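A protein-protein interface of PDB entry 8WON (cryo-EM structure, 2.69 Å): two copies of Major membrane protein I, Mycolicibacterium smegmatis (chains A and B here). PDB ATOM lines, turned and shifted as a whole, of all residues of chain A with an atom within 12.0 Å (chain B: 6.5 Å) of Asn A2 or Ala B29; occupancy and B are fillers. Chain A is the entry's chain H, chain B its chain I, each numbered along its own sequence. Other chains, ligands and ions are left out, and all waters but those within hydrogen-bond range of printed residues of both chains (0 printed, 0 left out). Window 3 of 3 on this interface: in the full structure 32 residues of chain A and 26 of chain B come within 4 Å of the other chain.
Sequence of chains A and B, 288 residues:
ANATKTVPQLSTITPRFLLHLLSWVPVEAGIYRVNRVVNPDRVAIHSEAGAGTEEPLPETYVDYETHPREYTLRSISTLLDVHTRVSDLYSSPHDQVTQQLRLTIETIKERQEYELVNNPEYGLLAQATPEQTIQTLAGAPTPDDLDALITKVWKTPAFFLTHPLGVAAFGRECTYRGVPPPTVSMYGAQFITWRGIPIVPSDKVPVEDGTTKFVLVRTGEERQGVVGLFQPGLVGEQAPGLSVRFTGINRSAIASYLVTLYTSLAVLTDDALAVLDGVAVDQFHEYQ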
ATOM      1  N   ALA A   1      30.580  -4.956  18.772  1.00  0.00           N
ATOM      2  CA  ALA A   1      29.504  -4.099  18.290  1.00  0.00           C
ATOM      3  C   ALA A   1      28.204  -4.367  19.044  1.00  0.00           C
ATOM      4  O   ALA A   1      28.165  -4.325  20.273  1.00  0.00           O
ATOM      5  CB  ALA A   1      29.301  -4.294  16.795  1.00  0.00           C
ATOM      6  N   ASN A   2      27.137  -4.634  18.295  1.00  0.00           N
ATOM      7  CA  ASN A   2      25.852  -4.933  18.906  1.00  0.00           C
ATOM      8  C   ASN A   2      25.853  -6.326  19.518  1.00  0.00           C
ATOM      9  O   ASN A   2      26.557  -7.228  19.057  1.00  0.00           O
ATOM     10  CB  ASN A   2      24.734  -4.821  17.871  1.00  0.00           C
ATOM     11  CG  ASN A   2      25.000  -3.746  16.840  1.00  0.00           C
ATOM     12  OD1 ASN A   2      25.046  -2.559  17.160  1.00  0.00           O
ATOM     13  ND2 ASN A   2      25.180  -4.157  15.594  1.00  0.00           N
ATOM     14  N   ALA A   3      25.064  -6.494  20.572  1.00  0.00           N
ATOM     15  CA  ALA A   3      24.800  -7.793  21.173  1.00  0.00           C
ATOM     16  C   ALA A   3      23.301  -8.036  21.188  1.00  0.00           C
ATOM     17  O   ALA A   3      22.527  -7.146  21.546  1.00  0.00           O
ATOM     18  CB  ALA A   3      25.355  -7.874  22.595  1.00  0.00           C
ATOM     19  N   THR A   4      22.893  -9.231  20.784  1.00  0.00           N
ATOM     20  CA  THR A   4      21.488  -9.602  20.876  1.00  0.00           C
ATOM     21  C   THR A   4      21.129  -9.821  22.338  1.00  0.00           C
ATOM     22  O   THR A   4      21.798 -10.584  23.041  1.00  0.00           O
ATOM     23  CB  THR A   4      21.206 -10.852  20.053  1.00  0.00           C
ATOM     24  OG1 THR A   4      21.472 -10.585  18.675  1.00  0.00           O
ATOM     25  CG2 THR A   4      19.758 -11.260  20.196  1.00  0.00           C
ATOM     26  N   LYS A   5      20.090  -9.141  22.805  1.00  0.00           N
ATOM     27  CA  LYS A   5      19.701  -9.157  24.204  1.00  0.00           C
ATOM     28  C   LYS A   5      18.408  -9.940  24.386  1.00  0.00           C
ATOM     29  O   LYS A   5      17.768 -10.376  23.427  1.00  0.00           O
ATOM     30  CB  LYS A   5      19.534  -7.732  24.734  1.00  0.00           C
ATOM     31  CG  LYS A   5      20.771  -7.161  25.398  1.00  0.00           C
ATOM     32  CD  LYS A   5      21.367  -6.038  24.564  1.00  0.00           C
ATOM     33  CE  LYS A   5      22.748  -5.651  25.060  1.00  0.00           C
ATOM     34  NZ  LYS A   5      23.292  -4.475  24.330  1.00  0.00           N
ATOM     35  N   THR A   6      18.037 -10.117  25.650  1.00  0.00           N
ATOM     36  CA  THR A   6      16.769 -10.715  26.033  1.00  0.00           C
ATOM     37  C   THR A   6      16.016  -9.761  26.946  1.00  0.00           C
ATOM     38  O   THR A   6      16.599  -8.882  27.584  1.00  0.00           O
ATOM     39  CB  THR A   6      16.959 -12.062  26.757  1.00  0.00           C
ATOM     40  OG1 THR A   6      17.560 -11.846  28.040  1.00  0.00           O
ATOM     41  CG2 THR A   6      17.826 -12.984  25.952  1.00  0.00           C
ATOM     42  N   SER A  91      18.314   0.615  27.238  1.00  0.00           N
ATOM     43  CA  SER A  91      18.554   1.460  26.072  1.00  0.00           C
ATOM     44  C   SER A  91      17.523   2.569  25.893  1.00  0.00           C
ATOM     45  O   SER A  91      17.687   3.420  25.014  1.00  0.00           O
ATOM     46  CB  SER A  91      18.614   0.611  24.799  1.00  0.00           C
ATOM     47  OG  SER A  91      17.309   0.270  24.364  1.00  0.00           O
ATOM     48  N   VAL B  27      21.654 -14.802  16.288  1.00  0.00           N
ATOM     49  CA  VAL B  27      22.469 -13.800  16.959  1.00  0.00           C
ATOM     50  C   VAL B  27      23.191 -13.017  15.874  1.00  0.00           C
ATOM     51  O   VAL B  27      24.066 -13.558  15.189  1.00  0.00           O
ATOM     52  CB  VAL B  27      23.465 -14.429  17.938  1.00  0.00           C
ATOM     53  CG1 VAL B  27      24.209 -13.356  18.672  1.00  0.00           C
ATOM     54  CG2 VAL B  27      22.744 -15.336  18.912  1.00  0.00           C
ATOM     55  N   GLU B  28      22.841 -11.742  15.726  1.00  0.00           N
ATOM     56  CA  GLU B  28      23.305 -10.971  14.582  1.00  0.00           C
ATOM     57  C   GLU B  28      24.727 -10.447  14.733  1.00  0.00           C
ATOM     58  O   GLU B  28      25.268  -9.906  13.764  1.00  0.00           O
ATOM     59  CB  GLU B  28      22.347  -9.809  14.316  1.00  0.00           C
ATOM     60  CG  GLU B  28      20.884 -10.229  14.283  1.00  0.00           C
ATOM     61  CD  GLU B  28      20.428 -10.649  12.898  1.00  0.00           C
ATOM     62  OE1 GLU B  28      21.152 -10.367  11.919  1.00  0.00           O
ATOM     63  OE2 GLU B  28      19.350 -11.270  12.789  1.00  0.00           O
ATOM     64  N   ALA B  29      25.348 -10.586  15.906  1.00  0.00           N
ATOM     65  CA  ALA B  29      26.740 -10.173  16.039  1.00  0.00           C
ATOM     66  C   ALA B  29      27.559 -11.136  16.894  1.00  0.00           C
ATOM     67  O   ALA B  29      28.646 -10.770  17.354  1.00  0.00           O
ATOM     68  CB  ALA B  29      26.836  -8.766  16.615  1.00  0.00           C
ATOM     69  N   GLY B  30      27.068 -12.351  17.121  1.00  0.00           N
ATOM     70  CA  GLY B  30      27.821 -13.361  17.827  1.00  0.00           C
ATOM     71  C   GLY B  30      27.800 -13.259  19.333  1.00  0.00           C
ATOM     72  O   GLY B  30      28.471 -14.057  19.992  1.00  0.00           O
ATOM     73  N   ILE B  31      27.057 -12.313  19.900  1.00  0.00           N
ATOM     74  CA  ILE B  31      26.985 -12.115  21.341  1.00  0.00           C
ATOM     75  C   ILE B  31      25.528 -12.182  21.767  1.00  0.00           C
ATOM     76  O   ILE B  31      24.669 -11.532  21.164  1.00  0.00           O
ATOM     77  CB  ILE B  31      27.612 -10.776  21.768  1.00  0.00           C
ATOM     78  CG1 ILE B  31      29.052 -10.678  21.266  1.00  0.00           C
ATOM     79  CG2 ILE B  31      27.555 -10.629  23.277  1.00  0.00           C
ATOM     80  CD1 ILE B  31      30.084 -11.144  22.254  1.00  0.00           C
ATOM     81  N   ARG B  33      23.122 -11.921  25.315  1.00  0.00           N
ATOM     82  CA  ARG B  33      23.078 -11.539  26.718  1.00  0.00           C
ATOM     83  C   ARG B  33      21.769 -12.018  27.321  1.00  0.00           C
ATOM     84  O   ARG B  33      20.698 -11.791  26.749  1.00  0.00           O
ATOM     85  CB  ARG B  33      23.228 -10.026  26.885  1.00  0.00           C
ATOM     86  CG  ARG B  33      23.612  -9.597  28.288  1.00  0.00           C
ATOM     87  CD  ARG B  33      24.414  -8.308  28.269  1.00  0.00           C
ATOM     88  NE  ARG B  33      25.409  -8.308  27.205  1.00  0.00           N
ATOM     89  CZ  ARG B  33      25.889  -7.214  26.630  1.00  0.00           C
ATOM     90  NH1 ARG B  33      25.487  -6.008  26.992  1.00  0.00           N
ATOM     91  NH2 ARG B  33      26.797  -7.335  25.665  1.00  0.00           N
ATOM     92  N   LEU B  73      29.309 -16.956  20.400  1.00  0.00           N
ATOM     93  CA  LEU B  73      29.291 -18.133  19.541  1.00  0.00           C
ATOM     94  C   LEU B  73      30.704 -18.616  19.256  1.00  0.00           C
ATOM     95  O   LEU B  73      31.611 -17.821  19.006  1.00  0.00           O
ATOM     96  CB  LEU B  73      28.582 -17.825  18.225  1.00  0.00           C
ATOM     97  CG  LEU B  73      27.174 -17.243  18.253  1.00  0.00           C
ATOM     98  CD1 LEU B  73      26.522 -17.361  16.906  1.00  0.00           C
ATOM     99  CD2 LEU B  73      26.348 -17.938  19.280  1.00  0.00           C
ATOM    100  N   GLN B 231      24.497 -17.756  13.923  1.00  0.00           N
ATOM    101  CA  GLN B 231      24.773 -16.460  13.321  1.00  0.00           C
ATOM    102  C   GLN B 231      24.232 -16.420  11.903  1.00  0.00           C
ATOM    103  O   GLN B 231      24.626 -17.259  11.082  1.00  0.00           O
ATOM    104  CB  GLN B 231      26.270 -16.190  13.317  1.00  0.00           C
ATOM    105  CG  GLN B 231      26.657 -14.888  12.662  1.00  0.00           C
ATOM    106  CD  GLN B 231      27.706 -14.145  13.445  1.00  0.00           C
ATOM    107  OE1 GLN B 231      28.655 -14.741  13.951  1.00  0.00           O
ATOM    108  NE2 GLN B 231      27.542 -12.836  13.556  1.00  0.00           N
ATOM    109  N   PRO B 232      23.351 -15.487  11.566  1.00  0.00           N
ATOM    110  CA  PRO B 232      22.836 -15.396  10.200  1.00  0.00           C
ATOM    111  C   PRO B 232      23.664 -14.449   9.338  1.00  0.00           C
ATOM    112  O   PRO B 232      24.550 -13.738   9.814  1.00  0.00           O
ATOM    113  CB  PRO B 232      21.419 -14.850  10.409  1.00  0.00           C
ATOM    114  CG  PRO B 232      21.477 -14.112  11.720  1.00  0.00           C
ATOM    115  CD  PRO B 232      22.747 -14.466  12.435  1.00  0.00           C
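The side-chain hydroxyl (OG1) of Thr A4 sits at hydrogen-bond distance from the backbone NH (N) of Glu B28, 3.5 Å away. N of Thr A4 is in hydrogen-bond range of O of Ile B31 (2.9 Å). O of Arg B33 sits close to N of Thr A6 (3.3 Å). O of Thr A4 sits at hydrogen-bond distance from N of Arg B33, at 3.0 Å.
Asn A2 touches just one residue of chain B: Ala B29. Of chain A, only Asn A2 comes within 4 Å of Ala B29. Val B27 touches one residue of chain A. Of chain A, only Thr A4 (3.5 Å) comes within 4 Å of Glu B28. No residue of chain A comes within 4 Å of Gly B30. Printed residues of chain A within 4 Å of Ile B31: Ala A3 (3.6 Å) and Thr A4 (2.9 Å). Of the printed residues of chain B, Ala A3 touches Ile B31 (3.6 Å) and Arg B33 (3.4 Å). Printed residues of chain B within 4 Å of Lys A5: Arg B33. Printed residues of chain B within 4 Å of Thr A4: Val B27, Glu B28, Ile B31 and Arg B33. Of the printed residues of chain B, Thr A6 touches Arg B33. Of the printed residues of chain A, Arg B33 touches Ala A3, Thr A4, Lys A5 and Thr A6. Ser A91 touches none of the printed residues of chain B. Leu B73 touches none of the printed residues of chain A. The nearest printed residue of chain B that does not touch Thr A6 is Ile B31 (8.1 Å).
Hydrophobic or aromatic side chains of chain A that line the printed part of chain B: Ala A3. Along chain A the printed residues that touch a printed residue of chain B span positions 2 to 6.
Among the printed residues, merely in contact across the chains: Asn A2 with Ala B29, Ala A3 with Ile B31, Ala A3 with Arg B33, Thr A4 with Val B27 and Lys A5 with Arg B33.
No position is printed for both chains. Of the 9 pairs that touch across the chains among the printed residues, none has its exchanged pair printed and touching as well.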
